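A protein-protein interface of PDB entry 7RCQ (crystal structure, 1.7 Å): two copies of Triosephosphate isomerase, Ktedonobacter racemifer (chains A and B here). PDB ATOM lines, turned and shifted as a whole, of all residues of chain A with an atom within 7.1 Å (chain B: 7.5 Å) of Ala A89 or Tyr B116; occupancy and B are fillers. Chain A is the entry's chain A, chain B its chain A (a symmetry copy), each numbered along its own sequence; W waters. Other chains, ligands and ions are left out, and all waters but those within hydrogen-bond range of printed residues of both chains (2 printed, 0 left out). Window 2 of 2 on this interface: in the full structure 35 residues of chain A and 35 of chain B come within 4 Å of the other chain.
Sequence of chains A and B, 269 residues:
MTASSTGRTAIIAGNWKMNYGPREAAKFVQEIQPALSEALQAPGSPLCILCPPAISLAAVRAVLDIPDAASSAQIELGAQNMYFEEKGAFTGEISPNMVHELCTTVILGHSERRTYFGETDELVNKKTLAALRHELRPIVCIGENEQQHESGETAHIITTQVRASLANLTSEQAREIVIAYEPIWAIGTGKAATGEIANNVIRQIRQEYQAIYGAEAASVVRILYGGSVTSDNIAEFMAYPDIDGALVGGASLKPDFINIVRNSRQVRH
The backbone NH (N) of Gly A88 is in hydrogen-bond range of the backbone carbonyl oxygen (O) of Met B18, at 2.9 Å.
The backbone NH (N) of Phe A90 is in hydrogen-bond range of the side-chain carboxylate (OE1) of Glu B112 (3.5 Å).
ND1 of His B110 lies within hydrogen-bond range of OG1 of Thr A91 (3.4 Å).
The side-chain hydroxyl (OG1) of Thr A91 is in hydrogen-bond range of the side-chain carboxylate (OE1) of Glu B112, 2.7 Å away.
NH1 of Arg B113 lies within hydrogen-bond range of O of Thr A91, at 2.9 Å.
OE1 of Glu B112 sits close to O of Ala A89 (3.1 Å).
The side-chain amide nitrogen (ND2) of Asn B19 is in hydrogen-bond range of the backbone carbonyl oxygen (O) of Trp B16.
NZ of Lys B17 lies within salt-bridge range of OE2 of Glu B112 (2.8 Å).
A ring nitrogen (ND1) of His B110 sits at hydrogen-bond distance from the backbone NH (N) of Glu B112 (3.0 Å).
The side-chain hydroxyl of Thr B115 is in hydrogen-bond range of the backbone carbonyl oxygen of Glu B112 (3.4 Å).
The backbone carbonyl oxygen (O) of Arg B113 lies within hydrogen-bond range of the backbone NH (N) of Gly B118, 3.1 Å away.
The guanidinium group (NE) of Arg B113 lies within salt-bridge range of the side-chain carboxylate (OE2) of Glu B119 (2.8 Å).
Among the printed residues, merely in contact across the chains: Lys A87 with Met B18 (3.3 Å), Thr A91 with Lys B17 (3.5 Å), Gly A88 with Asn B19 (3.5 Å), Gly A88 with Lys B17 (3.6 Å), Ala A89 with Lys B17 (3.7 Å), Phe A90 with Met B18 (3.7 Å), Phe A90 with Tyr B116 (3.7 Å), Tyr A83 with Phe B117 (3.7 Å), Ala A89 with Tyr B116 (3.8 Å), Tyr A83 with Met B18 (3.9 Å) and Lys A87 with Asn B19 (3.9 Å).
Of the printed residues of chain B, Ala A89 touches Lys B17, Glu B112 and Tyr B116.
Of chain A, only Ala A89 (3.8 Å) and Phe A90 (3.7 Å) come within 4 Å of Tyr B116.
Printed residues of chain B within 4 Å of Gly A88: Lys B17, Met B18 and Asn B19.
Of the printed residues of chain B, Lys A87 touches Met B18 and Asn B19.
Of the printed residues of chain A, Arg B113 touches Thr A91 (2.9 Å).
The nearest residue of chain B that does not touch Ala A89 is Asn B19 (4.9 Å).
The nearest printed residue of chain B that does not touch Lys A87 is Lys B17 (7.1 Å).
Printed residues of chain A that touch a printed residue of chain B: Tyr A83, Lys A87, Gly A88, Ala A89, Phe A90 and Thr A91.
Hydrophobic or aromatic side chains of chain A within 4 Å of the printed part of chain B: Tyr A83, Ala A89 and Phe A90.
Along chain A the printed residues that touch a printed residue of chain B span positions 83 to 91.
Of the 16 printed residues of chain B, 8 touch a printed residue of chain A.
Among the printed residues, no Asp or Glu carboxylate lies within 4 Å of a Lys or Arg side-chain nitrogen of the other chain.
Position printed for both chains: 117.
Water W1 bridges the side-chain hydroxyl of Tyr B116 and the backbone carbonyl oxygen of Ala A89.
Water W2 lies within hydrogen-bond range of ND2 of Asn B19 (3.0 Å), N of Ala A89 (3.2 Å) and O of Gly A88 (3.5 Å).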
ATOM      1  N   TYR A  83     -18.780  26.850   6.252  1.00  0.00           N
ATOM      2  CA  TYR A  83     -17.718  26.028   5.679  1.00  0.00           C
ATOM      3  C   TYR A  83     -17.378  26.526   4.269  1.00  0.00           C
ATOM      4  O   TYR A  83     -18.085  27.356   3.699  1.00  0.00           O
ATOM      5  CB  TYR A  83     -18.142  24.559   5.662  1.00  0.00           C
ATOM      6  CG  TYR A  83     -16.995  23.585   5.528  1.00  0.00           C
ATOM      7  CD1 TYR A  83     -15.918  23.625   6.396  1.00  0.00           C
ATOM      8  CD2 TYR A  83     -17.000  22.615   4.537  1.00  0.00           C
ATOM      9  CE1 TYR A  83     -14.859  22.720   6.274  1.00  0.00           C
ATOM     10  CE2 TYR A  83     -15.958  21.715   4.415  1.00  0.00           C
ATOM     11  CZ  TYR A  83     -14.892  21.772   5.278  1.00  0.00           C
ATOM     12  OH  TYR A  83     -13.855  20.862   5.144  1.00  0.00           O
ATOM     13  N   LYS A  87     -20.934  22.373  -1.238  1.00  0.00           N
ATOM     14  CA  LYS A  87     -21.947  21.428  -0.771  1.00  0.00           C
ATOM     15  C   LYS A  87     -21.211  20.138  -0.436  1.00  0.00           C
ATOM     16  O   LYS A  87     -20.046  19.963  -0.804  1.00  0.00           O
ATOM     17  CB  LYS A  87     -23.023  21.190  -1.830  1.00  0.00           C
ATOM     18  CG  LYS A  87     -22.502  20.555  -3.116  1.00  0.00           C
ATOM     19  CD  LYS A  87     -23.651  20.083  -3.999  1.00  0.00           C
ATOM     20  CE  LYS A  87     -23.156  19.278  -5.189  1.00  0.00           C
ATOM     21  NZ  LYS A  87     -21.992  18.420  -4.832  1.00  0.00           N
ATOM     22  N   GLY A  88     -21.889  19.244   0.270  1.00  0.00           N
ATOM     23  CA  GLY A  88     -21.370  17.895   0.360  1.00  0.00           C
ATOM     24  C   GLY A  88     -21.417  17.331   1.767  1.00  0.00           C
ATOM     25  O   GLY A  88     -22.182  17.777   2.623  1.00  0.00           O
ATOM     26  N   ALA A  89     -20.566  16.329   1.972  1.00  0.00           N
ATOM     27  CA  ALA A  89     -20.669  15.417   3.111  1.00  0.00           C
ATOM     28  C   ALA A  89     -19.886  15.991   4.293  1.00  0.00           C
ATOM     29  O   ALA A  89     -18.828  15.503   4.702  1.00  0.00           O
ATOM     30  CB  ALA A  89     -20.177  14.027   2.718  1.00  0.00           C
ATOM     31  N   PHE A  90     -20.445  17.069   4.844  1.00  0.00           N
ATOM     32  CA  PHE A  90     -19.866  17.772   5.992  1.00  0.00           C
ATOM     33  C   PHE A  90     -20.991  17.997   6.999  1.00  0.00           C
ATOM     34  O   PHE A  90     -21.523  19.101   7.110  1.00  0.00           O
ATOM     35  CB  PHE A  90     -19.198  19.074   5.544  1.00  0.00           C
ATOM     36  CG  PHE A  90     -18.253  18.877   4.397  1.00  0.00           C
ATOM     37  CD1 PHE A  90     -17.000  18.339   4.618  1.00  0.00           C
ATOM     38  CD2 PHE A  90     -18.642  19.179   3.100  1.00  0.00           C
ATOM     39  CE1 PHE A  90     -16.124  18.126   3.560  1.00  0.00           C
ATOM     40  CE2 PHE A  90     -17.768  18.975   2.033  1.00  0.00           C
ATOM     41  CZ  PHE A  90     -16.512  18.443   2.268  1.00  0.00           C
ATOM     42  N   THR A  91     -21.352  16.927   7.719  1.00  0.00           N
ATOM     43  CA  THR A  91     -22.476  16.984   8.650  1.00  0.00           C
ATOM     44  C   THR A  91     -22.292  18.122   9.651  1.00  0.00           C
ATOM     45  O   THR A  91     -21.233  18.248  10.274  1.00  0.00           O
ATOM     46  CB  THR A  91     -22.605  15.638   9.381  1.00  0.00           C
ATOM     47  OG1 THR A  91     -22.937  14.613   8.430  1.00  0.00           O
ATOM     48  CG2 THR A  91     -23.709  15.687  10.414  1.00  0.00           C
ATOM     49  N   PHE A 117     -12.508  25.405  18.651  1.00  0.00           N
ATOM     50  CA  PHE A 117     -12.834  24.473  17.583  1.00  0.00           C
ATOM     51  C   PHE A 117     -11.681  24.322  16.595  1.00  0.00           C
ATOM     52  O   PHE A 117     -11.869  23.794  15.494  1.00  0.00           O
ATOM     53  CB  PHE A 117     -14.143  24.901  16.912  1.00  0.00           C
ATOM     54  CG  PHE A 117     -15.266  25.125  17.902  1.00  0.00           C
ATOM     55  CD1 PHE A 117     -15.812  24.049  18.601  1.00  0.00           C
ATOM     56  CD2 PHE A 117     -15.755  26.393  18.161  1.00  0.00           C
ATOM     57  CE1 PHE A 117     -16.829  24.242  19.526  1.00  0.00           C
ATOM     58  CE2 PHE A 117     -16.765  26.600  19.095  1.00  0.00           C
ATOM     59  CZ  PHE A 117     -17.306  25.519  19.779  1.00  0.00           C
ATOM     60  N   LEU A 123      -7.552  27.388   7.213  1.00  0.00           N
ATOM     61  CA  LEU A 123      -8.983  27.145   7.053  1.00  0.00           C
ATOM     62  C   LEU A 123      -9.741  28.458   6.945  1.00  0.00           C
ATOM     63  O   LEU A 123     -10.673  28.581   6.145  1.00  0.00           O
ATOM     64  CB  LEU A 123      -9.505  26.305   8.225  1.00  0.00           C
ATOM     65  CG  LEU A 123     -11.020  26.158   8.359  1.00  0.00           C
ATOM     66  CD1 LEU A 123     -11.580  25.310   7.204  1.00  0.00           C
ATOM     67  CD2 LEU A 123     -11.414  25.565   9.717  1.00  0.00           C
ATOM     68  N   TRP B  16     -29.192  15.129   5.762  1.00  0.00           N
ATOM     69  CA  TRP B  16     -28.917  15.811   4.495  1.00  0.00           C
ATOM     70  C   TRP B  16     -27.467  16.274   4.358  1.00  0.00           C
ATOM     71  O   TRP B  16     -27.036  16.599   3.239  1.00  0.00           O
ATOM     72  CB  TRP B  16     -29.818  17.035   4.338  1.00  0.00           C
ATOM     73  CG  TRP B  16     -31.303  16.779   4.333  1.00  0.00           C
ATOM     74  CD1 TRP B  16     -31.960  15.611   4.628  1.00  0.00           C
ATOM     75  CD2 TRP B  16     -32.308  17.744   4.046  1.00  0.00           C
ATOM     76  NE1 TRP B  16     -33.325  15.800   4.519  1.00  0.00           N
ATOM     77  CE2 TRP B  16     -33.559  17.106   4.169  1.00  0.00           C
ATOM     78  CE3 TRP B  16     -32.270  19.089   3.665  1.00  0.00           C
ATOM     79  CZ2 TRP B  16     -34.763  17.773   3.936  1.00  0.00           C
ATOM     80  CZ3 TRP B  16     -33.465  19.751   3.443  1.00  0.00           C
ATOM     81  CH2 TRP B  16     -34.693  19.095   3.581  1.00  0.00           C
ATOM     82  N   LYS B  17     -26.726  16.338   5.459  1.00  0.00           N
ATOM     83  CA  LYS B  17     -25.360  16.888   5.488  1.00  0.00           C
ATOM     84  C   LYS B  17     -25.426  18.307   4.937  1.00  0.00           C
ATOM     85  O   LYS B  17     -26.417  19.021   5.155  1.00  0.00           O
ATOM     86  CB  LYS B  17     -24.392  15.967   4.766  1.00  0.00           C
ATOM     87  CG  LYS B  17     -24.479  14.552   5.321  1.00  0.00           C
ATOM     88  CD  LYS B  17     -23.388  13.640   4.788  1.00  0.00           C
ATOM     89  CE  LYS B  17     -23.592  12.220   5.342  1.00  0.00           C
ATOM     90  NZ  LYS B  17     -22.500  11.323   4.892  1.00  0.00           N
ATOM     91  N   MET B  18     -24.378  18.767   4.262  1.00  0.00           N
ATOM     92  CA  MET B  18     -24.370  20.186   3.891  1.00  0.00           C
ATOM     93  C   MET B  18     -24.882  20.305   2.454  1.00  0.00           C
ATOM     94  O   MET B  18     -24.175  20.526   1.470  1.00  0.00           O
ATOM     95  CB  MET B  18     -23.004  20.828   4.186  1.00  0.00           C
ATOM     96  CG  MET B  18     -22.774  22.225   3.598  1.00  0.00           C
ATOM     97  SD  MET B  18     -21.128  22.870   3.869  1.00  0.00           S
ATOM     98  CE  MET B  18     -20.421  22.624   2.237  1.00  0.00           C
ATOM     99  N   ASN B  19     -26.201  20.102   2.380  1.00  0.00           N
ATOM    100  CA  ASN B  19     -26.979  20.135   1.151  1.00  0.00           C
ATOM    101  C   ASN B  19     -28.345  20.723   1.439  1.00  0.00           C
ATOM    102  O   ASN B  19     -28.989  20.345   2.425  1.00  0.00           O
ATOM    103  CB  ASN B  19     -27.185  18.734   0.567  1.00  0.00           C
ATOM    104  CG  ASN B  19     -25.889  18.078   0.172  1.00  0.00           C
ATOM    105  OD1 ASN B  19     -25.414  18.255  -0.960  1.00  0.00           O
ATOM    106  ND2 ASN B  19     -25.307  17.301   1.092  1.00  0.00           N
ATOM    107  N   HIS B 110     -21.309  12.558  14.544  1.00  0.00           N
ATOM    108  CA  HIS B 110     -21.109  12.043  13.200  1.00  0.00           C
ATOM    109  C   HIS B 110     -19.622  11.946  12.893  1.00  0.00           C
ATOM    110  O   HIS B 110     -18.830  12.802  13.302  1.00  0.00           O
ATOM    111  CB  HIS B 110     -21.782  12.926  12.153  1.00  0.00           C
ATOM    112  CG  HIS B 110     -21.961  12.226  10.845  1.00  0.00           C
ATOM    113  ND1 HIS B 110     -20.974  12.180   9.882  1.00  0.00           N
ATOM    114  CD2 HIS B 110     -22.985  11.476  10.377  1.00  0.00           C
ATOM    115  CE1 HIS B 110     -21.397  11.458   8.860  1.00  0.00           C
ATOM    116  NE2 HIS B 110     -22.616  11.025   9.131  1.00  0.00           N
ATOM    117  N   SER B 111     -19.243  10.893  12.155  1.00  0.00           N
ATOM    118  CA  SER B 111     -17.825  10.683  11.881  1.00  0.00           C
ATOM    119  C   SER B 111     -17.219  11.854  11.124  1.00  0.00           C
ATOM    120  O   SER B 111     -16.023  12.131  11.264  1.00  0.00           O
ATOM    121  CB  SER B 111     -17.623   9.377  11.109  1.00  0.00           C
ATOM    122  OG  SER B 111     -18.300   9.429   9.885  1.00  0.00           O
ATOM    123  N   GLU B 112     -18.019  12.569  10.332  1.00  0.00           N
ATOM    124  CA  GLU B 112     -17.465  13.722   9.637  1.00  0.00           C
ATOM    125  C   GLU B 112     -17.059  14.813  10.623  1.00  0.00           C
ATOM    126  O   GLU B 112     -16.076  15.530  10.387  1.00  0.00           O
ATOM    127  CB  GLU B 112     -18.473  14.238   8.607  1.00  0.00           C
ATOM    128  CG  GLU B 112     -18.541  13.344   7.375  1.00  0.00           C
ATOM    129  CD  GLU B 112     -19.891  13.341   6.677  1.00  0.00           C
ATOM    130  OE1 GLU B 112     -20.695  14.268   6.915  1.00  0.00           O
ATOM    131  OE2 GLU B 112     -20.132  12.418   5.859  1.00  0.00           O
ATOM    132  N   ARG B 113     -17.779  14.930  11.745  1.00  0.00           N
ATOM    133  CA  ARG B 113     -17.402  15.903  12.766  1.00  0.00           C
ATOM    134  C   ARG B 113     -16.246  15.401  13.629  1.00  0.00           C
ATOM    135  O   ARG B 113     -15.398  16.199  14.036  1.00  0.00           O
ATOM    136  CB  ARG B 113     -18.613  16.256  13.634  1.00  0.00           C
ATOM    137  CG  ARG B 113     -19.777  16.836  12.822  1.00  0.00           C
ATOM    138  CD  ARG B 113     -20.556  17.937  13.551  1.00  0.00           C
ATOM    139  NE  ARG B 113     -19.699  19.047  13.954  1.00  0.00           N
ATOM    140  CZ  ARG B 113     -19.380  20.079  13.177  1.00  0.00           C
ATOM    141  NH1 ARG B 113     -19.850  20.164  11.930  1.00  0.00           N
ATOM    142  NH2 ARG B 113     -18.598  21.050  13.656  1.00  0.00           N
ATOM    143  N   ARG B 114     -16.184  14.089  13.895  1.00  0.00           N
ATOM    144  CA  ARG B 114     -15.042  13.556  14.637  1.00  0.00           C
ATOM    145  C   ARG B 114     -13.750  13.690  13.845  1.00  0.00           C
ATOM    146  O   ARG B 114     -12.690  13.968  14.419  1.00  0.00           O
ATOM    147  CB  ARG B 114     -15.287  12.094  15.011  1.00  0.00           C
ATOM    148  CG  ARG B 114     -16.497  11.889  15.914  1.00  0.00           C
ATOM    149  CD  ARG B 114     -16.680  10.412  16.205  1.00  0.00           C
ATOM    150  NE  ARG B 114     -17.855  10.096  17.016  1.00  0.00           N
ATOM    151  CZ  ARG B 114     -17.822   9.798  18.316  1.00  0.00           C
ATOM    152  NH1 ARG B 114     -16.675   9.810  18.984  1.00  0.00           N
ATOM    153  NH2 ARG B 114     -18.938   9.480  18.953  1.00  0.00           N
ATOM    154  N   THR B 115     -13.813  13.498  12.529  1.00  0.00           N
ATOM    155  CA  THR B 115     -12.610  13.505  11.709  1.00  0.00           C
ATOM    156  C   THR B 115     -12.225  14.908  11.237  1.00  0.00           C
ATOM    157  O   THR B 115     -11.087  15.339  11.439  1.00  0.00           O
ATOM    158  CB  THR B 115     -12.793  12.574  10.508  1.00  0.00           C
ATOM    159  OG1 THR B 115     -13.939  12.972   9.755  1.00  0.00           O
ATOM    160  CG2 THR B 115     -13.003  11.159  10.978  1.00  0.00           C
ATOM    161  N   TYR B 116     -13.150  15.645  10.619  1.00  0.00           N
ATOM    162  CA  TYR B 116     -12.777  16.965  10.106  1.00  0.00           C
ATOM    163  C   TYR B 116     -12.723  18.037  11.185  1.00  0.00           C
ATOM    164  O   TYR B 116     -11.944  18.994  11.063  1.00  0.00           O
ATOM    165  CB  TYR B 116     -13.736  17.423   9.007  1.00  0.00           C
ATOM    166  CG  TYR B 116     -13.904  16.468   7.857  1.00  0.00           C
ATOM    167  CD1 TYR B 116     -12.819  15.778   7.326  1.00  0.00           C
ATOM    168  CD2 TYR B 116     -15.144  16.276   7.279  1.00  0.00           C
ATOM    169  CE1 TYR B 116     -12.985  14.904   6.252  1.00  0.00           C
ATOM    170  CE2 TYR B 116     -15.318  15.419   6.216  1.00  0.00           C
ATOM    171  CZ  TYR B 116     -14.245  14.737   5.704  1.00  0.00           C
ATOM    172  OH  TYR B 116     -14.450  13.881   4.641  1.00  0.00           O
ATOM    173  N   PHE B 117     -13.542  17.933  12.228  1.00  0.00           N
ATOM    174  CA  PHE B 117     -13.661  19.030  13.176  1.00  0.00           C
ATOM    175  C   PHE B 117     -13.259  18.604  14.585  1.00  0.00           C
ATOM    176  O   PHE B 117     -13.550  19.309  15.556  1.00  0.00           O
ATOM    177  CB  PHE B 117     -15.076  19.613  13.110  1.00  0.00           C
ATOM    178  CG  PHE B 117     -15.503  19.963  11.700  1.00  0.00           C
ATOM    179  CD1 PHE B 117     -14.886  21.013  11.020  1.00  0.00           C
ATOM    180  CD2 PHE B 117     -16.483  19.240  11.044  1.00  0.00           C
ATOM    181  CE1 PHE B 117     -15.254  21.334   9.720  1.00  0.00           C
ATOM    182  CE2 PHE B 117     -16.850  19.545   9.738  1.00  0.00           C
ATOM    183  CZ  PHE B 117     -16.235  20.598   9.074  1.00  0.00           C
ATOM    184  N   GLY B 118     -12.591  17.460  14.707  1.00  0.00           N
ATOM    185  CA  GLY B 118     -11.927  17.092  15.942  1.00  0.00           C
ATOM    186  C   GLY B 118     -12.816  16.766  17.122  1.00  0.00           C
ATOM    187  O   GLY B 118     -12.338  16.796  18.261  1.00  0.00           O
ATOM    188  N   GLU B 119     -14.086  16.439  16.899  1.00  0.00           N
ATOM    189  CA  GLU B 119     -14.961  16.140  18.026  1.00  0.00           C
ATOM    190  C   GLU B 119     -14.540  14.834  18.688  1.00  0.00           C
ATOM    191  O   GLU B 119     -14.213  13.855  18.019  1.00  0.00           O
ATOM    192  CB  GLU B 119     -16.423  16.065  17.573  1.00  0.00           C
ATOM    193  CG  GLU B 119     -16.872  17.383  16.942  1.00  0.00           C
ATOM    194  CD  GLU B 119     -18.365  17.676  17.077  1.00  0.00           C
ATOM    195  OE1 GLU B 119     -19.101  16.844  17.640  1.00  0.00           O
ATOM    196  OE2 GLU B 119     -18.791  18.740  16.578  1.00  0.00           O
ATOM    197  N   ILE B 187     -19.441   5.082   4.321  1.00  0.00           N
ATOM    198  CA  ILE B 187     -20.083   6.386   4.172  1.00  0.00           C
ATOM    199  C   ILE B 187     -19.755   6.958   2.799  1.00  0.00           C
ATOM    200  O   ILE B 187     -18.586   7.204   2.483  1.00  0.00           O
ATOM    201  CB  ILE B 187     -19.651   7.347   5.290  1.00  0.00           C
ATOM    202  CG1 ILE B 187     -20.022   6.761   6.649  1.00  0.00           C
ATOM    203  CG2 ILE B 187     -20.297   8.728   5.110  1.00  0.00           C
ATOM    204  CD1 ILE B 187     -19.546   7.585   7.816  1.00  0.00           C
ATOM    205  N   GLY B 188     -20.792   7.181   1.987  1.00  0.00           N
ATOM    206  CA  GLY B 188     -20.628   7.831   0.700  1.00  0.00           C
ATOM    207  C   GLY B 188     -19.842   7.046  -0.322  1.00  0.00           C
ATOM    208  O   GLY B 188     -19.693   7.517  -1.457  1.00  0.00           O
HETATM  209  O   HOH W   1     -16.841  13.933   3.653  1.00  0.00           O
HETATM  210  O   HOH W   2     -23.200  15.180   0.565  1.00  0.00           O
